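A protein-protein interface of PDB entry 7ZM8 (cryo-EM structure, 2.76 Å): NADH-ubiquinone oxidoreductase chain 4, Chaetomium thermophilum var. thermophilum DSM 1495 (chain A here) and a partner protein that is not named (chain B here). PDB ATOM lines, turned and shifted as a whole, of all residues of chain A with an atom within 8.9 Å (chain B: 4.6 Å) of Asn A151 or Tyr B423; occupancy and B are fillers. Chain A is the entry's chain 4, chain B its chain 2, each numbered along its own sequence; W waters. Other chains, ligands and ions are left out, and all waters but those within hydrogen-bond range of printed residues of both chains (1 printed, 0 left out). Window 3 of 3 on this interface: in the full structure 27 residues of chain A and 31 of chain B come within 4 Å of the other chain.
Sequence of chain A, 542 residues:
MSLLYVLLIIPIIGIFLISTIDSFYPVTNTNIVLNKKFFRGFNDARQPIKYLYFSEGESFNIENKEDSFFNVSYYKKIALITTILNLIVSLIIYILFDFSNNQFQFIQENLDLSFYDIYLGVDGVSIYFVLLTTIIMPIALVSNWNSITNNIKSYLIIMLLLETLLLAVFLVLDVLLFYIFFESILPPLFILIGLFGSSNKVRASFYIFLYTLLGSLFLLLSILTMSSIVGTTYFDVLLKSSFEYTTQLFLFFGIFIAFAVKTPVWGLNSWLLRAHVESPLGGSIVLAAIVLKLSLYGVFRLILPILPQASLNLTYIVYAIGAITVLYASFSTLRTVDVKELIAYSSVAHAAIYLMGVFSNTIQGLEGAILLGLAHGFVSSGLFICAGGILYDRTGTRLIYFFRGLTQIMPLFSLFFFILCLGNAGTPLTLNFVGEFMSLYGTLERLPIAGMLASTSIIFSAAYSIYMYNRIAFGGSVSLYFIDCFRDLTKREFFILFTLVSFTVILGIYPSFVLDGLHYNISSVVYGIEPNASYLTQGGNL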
ATOM      1  N   VAL A  72       0.370  20.895  -8.488  1.00  0.00           N
ATOM      2  CA  VAL A  72       1.387  21.931  -8.412  1.00  0.00           C
ATOM      3  C   VAL A  72       0.870  23.242  -8.970  1.00  0.00           C
ATOM      4  O   VAL A  72       1.388  24.305  -8.622  1.00  0.00           O
ATOM      5  CB  VAL A  72       2.675  21.510  -9.144  1.00  0.00           C
ATOM      6  CG1 VAL A  72       3.248  20.248  -8.531  1.00  0.00           C
ATOM      7  CG2 VAL A  72       2.413  21.321 -10.625  1.00  0.00           C
ATOM      8  N   TYR A  75      -0.347  25.274  -6.071  1.00  0.00           N
ATOM      9  CA  TYR A  75       0.765  25.848  -5.284  1.00  0.00           C
ATOM     10  C   TYR A  75       1.240  27.111  -5.977  1.00  0.00           C
ATOM     11  O   TYR A  75       1.663  28.054  -5.294  1.00  0.00           O
ATOM     12  CB  TYR A  75       1.948  24.883  -5.256  1.00  0.00           C
ATOM     13  CG  TYR A  75       1.778  23.608  -4.477  1.00  0.00           C
ATOM     14  CD1 TYR A  75       1.312  23.615  -3.177  1.00  0.00           C
ATOM     15  CD2 TYR A  75       2.135  22.393  -5.031  1.00  0.00           C
ATOM     16  CE1 TYR A  75       1.160  22.439  -2.464  1.00  0.00           C
ATOM     17  CE2 TYR A  75       1.992  21.209  -4.334  1.00  0.00           C
ATOM     18  CZ  TYR A  75       1.499  21.232  -3.043  1.00  0.00           C
ATOM     19  OH  TYR A  75       1.366  20.072  -2.339  1.00  0.00           O
ATOM     20  N   ILE A 148      10.566  24.941 -13.709  1.00  0.00           N
ATOM     21  CA  ILE A 148      11.064  24.329 -12.480  1.00  0.00           C
ATOM     22  C   ILE A 148      10.839  22.819 -12.490  1.00  0.00           C
ATOM     23  O   ILE A 148      11.794  22.036 -12.430  1.00  0.00           O
ATOM     24  CB  ILE A 148      10.431  25.008 -11.253  1.00  0.00           C
ATOM     25  CG1 ILE A 148      10.965  26.434 -11.134  1.00  0.00           C
ATOM     26  CG2 ILE A 148      10.729  24.236  -9.986  1.00  0.00           C
ATOM     27  CD1 ILE A 148      12.453  26.532 -11.294  1.00  0.00           C
ATOM     28  N   THR A 149       9.583  22.396 -12.578  1.00  0.00           N
ATOM     29  CA  THR A 149       9.261  20.943 -12.727  1.00  0.00           C
ATOM     30  C   THR A 149       9.404  20.103 -11.451  1.00  0.00           C
ATOM     31  O   THR A 149       8.481  19.329 -11.184  1.00  0.00           O
ATOM     32  CB  THR A 149       9.945  20.288 -13.942  1.00  0.00           C
ATOM     33  OG1 THR A 149      11.267  19.851 -13.618  1.00  0.00           O
ATOM     34  CG2 THR A 149       9.949  21.147 -15.190  1.00  0.00           C
ATOM     35  N   ASN A 150      10.504  20.210 -10.714  1.00  0.00           N
ATOM     36  CA  ASN A 150      10.734  19.341  -9.534  1.00  0.00           C
ATOM     37  C   ASN A 150      11.004  20.230  -8.325  1.00  0.00           C
ATOM     38  O   ASN A 150      11.588  21.293  -8.535  1.00  0.00           O
ATOM     39  CB  ASN A 150      11.880  18.370  -9.793  1.00  0.00           C
ATOM     40  CG  ASN A 150      12.103  17.376  -8.672  1.00  0.00           C
ATOM     41  OD1 ASN A 150      11.173  17.017  -7.951  1.00  0.00           O
ATOM     42  ND2 ASN A 150      13.334  16.917  -8.522  1.00  0.00           N
ATOM     43  N   ASN A 151      10.612  19.798  -7.122  1.00  0.00           N
ATOM     44  CA  ASN A 151      10.772  20.614  -5.893  1.00  0.00           C
ATOM     45  C   ASN A 151      10.083  21.974  -6.088  1.00  0.00           C
ATOM     46  O   ASN A 151      10.695  22.989  -5.804  1.00  0.00           O
ATOM     47  CB  ASN A 151      12.224  20.619  -5.403  1.00  0.00           C
ATOM     48  CG  ASN A 151      12.781  19.245  -5.123  1.00  0.00           C
ATOM     49  OD1 ASN A 151      12.180  18.465  -4.392  1.00  0.00           O
ATOM     50  ND2 ASN A 151      13.938  18.953  -5.688  1.00  0.00           N
ATOM     51  N   ILE A 152       8.819  21.981  -6.485  1.00  0.00           N
ATOM     52  CA  ILE A 152       8.162  23.268  -6.840  1.00  0.00           C
ATOM     53  C   ILE A 152       7.712  23.996  -5.580  1.00  0.00           C
ATOM     54  O   ILE A 152       7.914  25.208  -5.527  1.00  0.00           O
ATOM     55  CB  ILE A 152       7.025  23.060  -7.872  1.00  0.00           C
ATOM     56  CG1 ILE A 152       7.532  22.441  -9.174  1.00  0.00           C
ATOM     57  CG2 ILE A 152       6.254  24.343  -8.131  1.00  0.00           C
ATOM     58  CD1 ILE A 152       6.482  22.367 -10.251  1.00  0.00           C
ATOM     59  N   LYS A 153       7.191  23.284  -4.588  1.00  0.00           N
ATOM     60  CA  LYS A 153       6.842  23.928  -3.299  1.00  0.00           C
ATOM     61  C   LYS A 153       8.065  24.577  -2.678  1.00  0.00           C
ATOM     62  O   LYS A 153       7.976  25.725  -2.268  1.00  0.00           O
ATOM     63  CB  LYS A 153       6.395  22.875  -2.292  1.00  0.00           C
ATOM     64  CG  LYS A 153       4.981  22.347  -2.464  1.00  0.00           C
ATOM     65  CD  LYS A 153       4.548  21.461  -1.326  1.00  0.00           C
ATOM     66  CE  LYS A 153       4.584  22.161   0.012  1.00  0.00           C
ATOM     67  NZ  LYS A 153       4.169  21.256   1.106  1.00  0.00           N
ATOM     68  N   SER A 154       9.179  23.860  -2.648  1.00  0.00           N
ATOM     69  CA  SER A 154      10.431  24.398  -2.070  1.00  0.00           C
ATOM     70  C   SER A 154      10.833  25.649  -2.836  1.00  0.00           C
ATOM     71  O   SER A 154      11.197  26.627  -2.200  1.00  0.00           O
ATOM     72  CB  SER A 154      11.515  23.376  -2.092  1.00  0.00           C
ATOM     73  OG  SER A 154      11.943  23.125  -3.411  1.00  0.00           O
ATOM     74  N   TYR A 155      10.712  25.613  -4.150  1.00  0.00           N
ATOM     75  CA  TYR A 155      11.085  26.765  -4.960  1.00  0.00           C
ATOM     76  C   TYR A 155      10.213  27.971  -4.640  1.00  0.00           C
ATOM     77  O   TYR A 155      10.713  29.086  -4.475  1.00  0.00           O
ATOM     78  CB  TYR A 155      10.987  26.404  -6.443  1.00  0.00           C
ATOM     79  CG  TYR A 155      11.117  27.577  -7.383  1.00  0.00           C
ATOM     80  CD1 TYR A 155      12.359  28.045  -7.777  1.00  0.00           C
ATOM     81  CD2 TYR A 155       9.991  28.213  -7.877  1.00  0.00           C
ATOM     82  CE1 TYR A 155      12.470  29.118  -8.626  1.00  0.00           C
ATOM     83  CE2 TYR A 155      10.091  29.276  -8.724  1.00  0.00           C
ATOM     84  CZ  TYR A 155      11.329  29.728  -9.099  1.00  0.00           C
ATOM     85  OH  TYR A 155      11.420  30.793  -9.959  1.00  0.00           O
ATOM     86  N   LEU A 156       8.900  27.759  -4.544  1.00  0.00           N
ATOM     87  CA  LEU A 156       7.989  28.853  -4.238  1.00  0.00           C
ATOM     88  C   LEU A 156       8.200  29.394  -2.833  1.00  0.00           C
ATOM     89  O   LEU A 156       8.037  30.594  -2.600  1.00  0.00           O
ATOM     90  CB  LEU A 156       6.544  28.392  -4.411  1.00  0.00           C
ATOM     91  CG  LEU A 156       6.145  27.817  -5.767  1.00  0.00           C
ATOM     92  CD1 LEU A 156       4.856  27.047  -5.634  1.00  0.00           C
ATOM     93  CD2 LEU A 156       6.014  28.904  -6.807  1.00  0.00           C
ATOM     94  N   ILE A 157       8.538  28.523  -1.884  1.00  0.00           N
ATOM     95  CA  ILE A 157       8.721  28.953  -0.503  1.00  0.00           C
ATOM     96  C   ILE A 157       9.973  29.812  -0.369  1.00  0.00           C
ATOM     97  O   ILE A 157       9.999  30.777   0.402  1.00  0.00           O
ATOM     98  CB  ILE A 157       8.750  27.722   0.421  1.00  0.00           C
ATOM     99  CG1 ILE A 157       7.338  27.167   0.589  1.00  0.00           C
ATOM    100  CG2 ILE A 157       9.341  28.060   1.774  1.00  0.00           C
ATOM    101  CD1 ILE A 157       7.293  25.752   1.090  1.00  0.00           C
ATOM    102  N   ILE A 158      11.029  29.482  -1.114  1.00  0.00           N
ATOM    103  CA  ILE A 158      12.256  30.267  -1.045  1.00  0.00           C
ATOM    104  C   ILE A 158      12.040  31.665  -1.615  1.00  0.00           C
ATOM    105  O   ILE A 158      12.504  32.658  -1.043  1.00  0.00           O
ATOM    106  CB  ILE A 158      13.400  29.530  -1.762  1.00  0.00           C
ATOM    107  CG1 ILE A 158      13.827  28.307  -0.957  1.00  0.00           C
ATOM    108  CG2 ILE A 158      14.573  30.459  -1.984  1.00  0.00           C
ATOM    109  CD1 ILE A 158      14.546  27.257  -1.766  1.00  0.00           C
ATOM    110  N   ILE A 191      20.621  27.592  -1.398  1.00  0.00           N
ATOM    111  CA  ILE A 191      19.791  26.437  -1.707  1.00  0.00           C
ATOM    112  C   ILE A 191      18.961  26.650  -2.972  1.00  0.00           C
ATOM    113  O   ILE A 191      18.621  25.683  -3.660  1.00  0.00           O
ATOM    114  CB  ILE A 191      18.916  26.112  -0.485  1.00  0.00           C
ATOM    115  CG1 ILE A 191      19.762  25.420   0.583  1.00  0.00           C
ATOM    116  CG2 ILE A 191      17.718  25.257  -0.850  1.00  0.00           C
ATOM    117  CD1 ILE A 191      18.983  24.946   1.783  1.00  0.00           C
ATOM    118  N   LEU A 192      18.658  27.891  -3.335  1.00  0.00           N
ATOM    119  CA  LEU A 192      17.971  28.099  -4.632  1.00  0.00           C
ATOM    120  C   LEU A 192      18.893  27.631  -5.773  1.00  0.00           C
ATOM    121  O   LEU A 192      18.407  26.923  -6.656  1.00  0.00           O
ATOM    122  CB  LEU A 192      17.576  29.571  -4.790  1.00  0.00           C
ATOM    123  CG  LEU A 192      16.520  29.853  -5.853  1.00  0.00           C
ATOM    124  CD1 LEU A 192      15.199  29.198  -5.486  1.00  0.00           C
ATOM    125  CD2 LEU A 192      16.335  31.346  -6.037  1.00  0.00           C
ATOM    126  N   GLY A 194      21.653  25.606  -5.653  1.00  0.00           N
ATOM    127  CA  GLY A 194      21.934  24.171  -5.511  1.00  0.00           C
ATOM    128  C   GLY A 194      20.794  23.265  -5.913  1.00  0.00           C
ATOM    129  O   GLY A 194      21.087  22.236  -6.516  1.00  0.00           O
ATOM    130  N   LEU A 195      19.543  23.637  -5.638  1.00  0.00           N
ATOM    131  CA  LEU A 195      18.396  22.763  -5.982  1.00  0.00           C
ATOM    132  C   LEU A 195      17.917  23.002  -7.410  1.00  0.00           C
ATOM    133  O   LEU A 195      17.552  22.017  -8.049  1.00  0.00           O
ATOM    134  CB  LEU A 195      17.254  22.966  -4.986  1.00  0.00           C
ATOM    135  CG  LEU A 195      17.227  22.054  -3.762  1.00  0.00           C
ATOM    136  CD1 LEU A 195      16.156  22.515  -2.790  1.00  0.00           C
ATOM    137  CD2 LEU A 195      16.975  20.612  -4.164  1.00  0.00           C
ATOM    138  N   PHE A 196      17.906  24.240  -7.899  1.00  0.00           N
ATOM    139  CA  PHE A 196      17.269  24.525  -9.216  1.00  0.00           C
ATOM    140  C   PHE A 196      18.239  25.168 -10.194  1.00  0.00           C
ATOM    141  O   PHE A 196      17.788  25.713 -11.197  1.00  0.00           O
ATOM    142  CB  PHE A 196      16.020  25.386  -9.020  1.00  0.00           C
ATOM    143  CG  PHE A 196      15.226  25.052  -7.788  1.00  0.00           C
ATOM    144  CD1 PHE A 196      14.269  24.057  -7.818  1.00  0.00           C
ATOM    145  CD2 PHE A 196      15.449  25.717  -6.595  1.00  0.00           C
ATOM    146  CE1 PHE A 196      13.555  23.734  -6.678  1.00  0.00           C
ATOM    147  CE2 PHE A 196      14.732  25.395  -5.456  1.00  0.00           C
ATOM    148  CZ  PHE A 196      13.789  24.400  -5.502  1.00  0.00           C
ATOM    149  N   LYS A 201      26.397  24.437 -10.794  1.00  0.00           N
ATOM    150  CA  LYS A 201      25.654  25.029  -9.653  1.00  0.00           C
ATOM    151  C   LYS A 201      26.392  24.929  -8.315  1.00  0.00           C
ATOM    152  O   LYS A 201      26.289  25.880  -7.547  1.00  0.00           O
ATOM    153  CB  LYS A 201      24.280  24.352  -9.557  1.00  0.00           C
ATOM    154  CG  LYS A 201      24.272  22.855  -9.291  1.00  0.00           C
ATOM    155  CD  LYS A 201      22.876  22.307  -9.187  1.00  0.00           C
ATOM    156  CE  LYS A 201      22.844  20.855  -8.770  1.00  0.00           C
ATOM    157  NZ  LYS A 201      21.461  20.398  -8.500  1.00  0.00           N
ATOM    158  N   GLY B 420      21.009  13.351  -0.069  1.00  0.00           N
ATOM    159  CA  GLY B 420      19.578  13.240  -0.400  1.00  0.00           C
ATOM    160  C   GLY B 420      18.643  13.110   0.786  1.00  0.00           C
ATOM    161  O   GLY B 420      17.508  12.688   0.552  1.00  0.00           O
ATOM    162  N   TYR B 421      19.067  13.432   2.013  1.00  0.00           N
ATOM    163  CA  TYR B 421      18.087  13.407   3.114  1.00  0.00           C
ATOM    164  C   TYR B 421      16.929  14.378   2.940  1.00  0.00           C
ATOM    165  O   TYR B 421      15.889  14.126   3.524  1.00  0.00           O
ATOM    166  CB  TYR B 421      18.799  13.475   4.469  1.00  0.00           C
ATOM    167  CG  TYR B 421      17.991  12.839   5.569  1.00  0.00           C
ATOM    168  CD1 TYR B 421      17.927  11.463   5.695  1.00  0.00           C
ATOM    169  CD2 TYR B 421      17.240  13.606   6.440  1.00  0.00           C
ATOM    170  CE1 TYR B 421      17.167  10.865   6.683  1.00  0.00           C
ATOM    171  CE2 TYR B 421      16.473  13.024   7.432  1.00  0.00           C
ATOM    172  CZ  TYR B 421      16.435  11.649   7.553  1.00  0.00           C
ATOM    173  OH  TYR B 421      15.680  11.073   8.529  1.00  0.00           O
ATOM    174  N   PHE B 422      17.126  15.454   2.181  1.00  0.00           N
ATOM    175  CA  PHE B 422      16.028  16.416   1.903  1.00  0.00           C
ATOM    176  C   PHE B 422      14.842  15.645   1.327  1.00  0.00           C
ATOM    177  O   PHE B 422      13.696  15.918   1.708  1.00  0.00           O
ATOM    178  CB  PHE B 422      16.534  17.513   0.965  1.00  0.00           C
ATOM    179  CG  PHE B 422      15.489  18.470   0.455  1.00  0.00           C
ATOM    180  CD1 PHE B 422      14.762  19.262   1.330  1.00  0.00           C
ATOM    181  CD2 PHE B 422      15.253  18.596  -0.903  1.00  0.00           C
ATOM    182  CE1 PHE B 422      13.812  20.150   0.854  1.00  0.00           C
ATOM    183  CE2 PHE B 422      14.300  19.484  -1.377  1.00  0.00           C
ATOM    184  CZ  PHE B 422      13.587  20.261  -0.498  1.00  0.00           C
ATOM    185  N   TYR B 423      15.119  14.724   0.407  1.00  0.00           N
ATOM    186  CA  TYR B 423      14.052  13.886  -0.199  1.00  0.00           C
ATOM    187  C   TYR B 423      13.426  12.940   0.839  1.00  0.00           C
ATOM    188  O   TYR B 423      12.195  12.763   0.804  1.00  0.00           O
ATOM    189  CB  TYR B 423      14.596  13.253  -1.480  1.00  0.00           C
ATOM    190  CG  TYR B 423      15.144  14.278  -2.440  1.00  0.00           C
ATOM    191  CD1 TYR B 423      14.296  15.063  -3.203  1.00  0.00           C
ATOM    192  CD2 TYR B 423      16.505  14.499  -2.556  1.00  0.00           C
ATOM    193  CE1 TYR B 423      14.787  16.021  -4.074  1.00  0.00           C
ATOM    194  CE2 TYR B 423      17.012  15.453  -3.422  1.00  0.00           C
ATOM    195  CZ  TYR B 423      16.150  16.218  -4.184  1.00  0.00           C
ATOM    196  OH  TYR B 423      16.645  17.158  -5.041  1.00  0.00           O
ATOM    197  N   ILE B 424      14.242  12.327   1.703  1.00  0.00           N
ATOM    198  CA  ILE B 424      13.734  11.397   2.760  1.00  0.00           C
ATOM    199  C   ILE B 424      12.933  12.131   3.852  1.00  0.00           C
ATOM    200  O   ILE B 424      11.844  11.640   4.193  1.00  0.00           O
ATOM    201  CB  ILE B 424      14.899  10.567   3.335  1.00  0.00           C
ATOM    202  CG1 ILE B 424      15.621   9.781   2.239  1.00  0.00           C
ATOM    203  CG2 ILE B 424      14.432   9.664   4.464  1.00  0.00           C
ATOM    204  CD1 ILE B 424      16.778   8.954   2.740  1.00  0.00           C
ATOM    205  N   ASN B 425      13.425  13.271   4.354  1.00  0.00           N
ATOM    206  CA  ASN B 425      12.755  14.010   5.465  1.00  0.00           C
ATOM    207  C   ASN B 425      13.051  15.516   5.314  1.00  0.00           C
ATOM    208  O   ASN B 425      14.120  15.932   5.780  1.00  0.00           O
ATOM    209  CB  ASN B 425      13.110  13.441   6.839  1.00  0.00           C
ATOM    210  CG  ASN B 425      12.119  13.803   7.925  1.00  0.00           C
ATOM    211  OD1 ASN B 425      11.494  14.857   7.882  1.00  0.00           O
ATOM    212  ND2 ASN B 425      11.983  12.937   8.916  1.00  0.00           N
ATOM    213  N   PHE B 489      21.000  18.487   0.498  1.00  0.00           N
ATOM    214  CA  PHE B 489      20.004  19.073  -0.442  1.00  0.00           C
ATOM    215  C   PHE B 489      20.389  19.023  -1.925  1.00  0.00           C
ATOM    216  O   PHE B 489      19.465  19.007  -2.750  1.00  0.00           O
ATOM    217  CB  PHE B 489      19.760  20.543  -0.084  1.00  0.00           C
ATOM    218  CG  PHE B 489      19.165  20.823   1.273  1.00  0.00           C
ATOM    219  CD1 PHE B 489      19.954  20.829   2.412  1.00  0.00           C
ATOM    220  CD2 PHE B 489      17.822  21.133   1.406  1.00  0.00           C
ATOM    221  CE1 PHE B 489      19.407  21.098   3.656  1.00  0.00           C
ATOM    222  CE2 PHE B 489      17.276  21.405   2.649  1.00  0.00           C
ATOM    223  CZ  PHE B 489      18.068  21.389   3.773  1.00  0.00           C
ATOM    224  N   TYR B 491      21.845  16.665  -3.769  1.00  0.00           N
ATOM    225  CA  TYR B 491      21.960  15.347  -4.442  1.00  0.00           C
ATOM    226  C   TYR B 491      20.778  14.441  -4.109  1.00  0.00           C
ATOM    227  O   TYR B 491      20.127  14.674  -3.081  1.00  0.00           O
ATOM    228  CB  TYR B 491      23.263  14.655  -4.046  1.00  0.00           C
ATOM    229  CG  TYR B 491      24.512  15.469  -4.257  1.00  0.00           C
ATOM    230  CD1 TYR B 491      24.982  15.736  -5.532  1.00  0.00           C
ATOM    231  CD2 TYR B 491      25.229  15.965  -3.183  1.00  0.00           C
ATOM    232  CE1 TYR B 491      26.127  16.487  -5.734  1.00  0.00           C
ATOM    233  CE2 TYR B 491      26.378  16.714  -3.369  1.00  0.00           C
ATOM    234  CZ  TYR B 491      26.829  16.977  -4.649  1.00  0.00           C
ATOM    235  OH  TYR B 491      27.960  17.713  -4.841  1.00  0.00           O
ATOM    236  N   SER B 492      20.502  13.460  -4.970  1.00  0.00           N
ATOM    237  CA  SER B 492      19.467  12.471  -4.740  1.00  0.00           C
ATOM    238  C   SER B 492      19.941  11.440  -3.719  1.00  0.00           C
ATOM    239  O   SER B 492      21.138  11.166  -3.610  1.00  0.00           O
ATOM    240  CB  SER B 492      19.107  11.776  -6.041  1.00  0.00           C
ATOM    241  OG  SER B 492      18.544  12.696  -6.958  1.00  0.00           O
ATOM    242  N   PRO B 493      19.019  10.802  -2.941  1.00  0.00           N
ATOM    243  CA  PRO B 493      19.393   9.810  -1.934  1.00  0.00           C
ATOM    244  C   PRO B 493      19.820   8.412  -2.391  1.00  0.00           C
ATOM    245  O   PRO B 493      19.169   7.837  -3.237  1.00  0.00           O
ATOM    246  CB  PRO B 493      18.147   9.656  -1.058  1.00  0.00           C
ATOM    247  CG  PRO B 493      17.002   9.929  -1.986  1.00  0.00           C
ATOM    248  CD  PRO B 493      17.542  10.977  -2.929  1.00  0.00           C
HETATM  249  O   HOH W   1      18.981  19.040  -6.594  1.00  0.00           O
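Phe B422 touches Asn A151 (CE2 to OD1, 3.8 Å). CE2 of Phe B422 touches CD1 of Leu A195, at 3.8 Å. CD2 of Leu A195 touches OH of Tyr B423, at 3.6 Å. Leu A195 touches Phe B489 (CD2 to O, 3.3 Å).
Water W1 lies within hydrogen-bond range of OH of Tyr B423 (3.4 Å) and NZ of Lys A201 (3.4 Å).
The backbone carbonyl oxygen of Asn A151 lies within hydrogen-bond range of the side-chain hydroxyl of Ser A154 (2.7 Å).
Thr A149 touches none of the printed residues of chain B. Asn A151 touches just these residues of chain B: Phe B422 (3.8 Å) and Tyr B423 (3.3 Å). Tyr A155 touches none of the printed residues of chain B. Printed residues of chain B within 4 Å of Leu A195: Phe B422, Tyr B423 and Phe B489. Of the printed residues of chain A, Phe B422 touches Asn A151 (3.8 Å) and Leu A195 (3.8 Å). Tyr B423 touches just these residues of chain A: Asn A151 (3.3 Å) and Leu A195 (3.6 Å). Printed residues of chain A within 4 Å of Phe B489: Leu A195 (3.3 Å). The nearest residue of chain A that does not touch Tyr B423 is Asn A150 (4.8 Å). The nearest printed residue of chain A that does not touch Phe B422 is Ser A154 (4.1 Å).
The side-chain amide nitrogen of Asn A151 is in hydrogen-bond range of the side-chain hydroxyl of Tyr B423.
Hydrophobic or aromatic side chains of chain A within 4 Å of the printed part of chain B: Leu A195. Hydrophobic or aromatic side chains of chain B within 4 Å of the printed part of chain A: Phe B422 and Tyr B423. Among the printed residues, no Asp or Glu carboxylate lies within 4 Å of a Lys or Arg side-chain nitrogen of the other chain.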
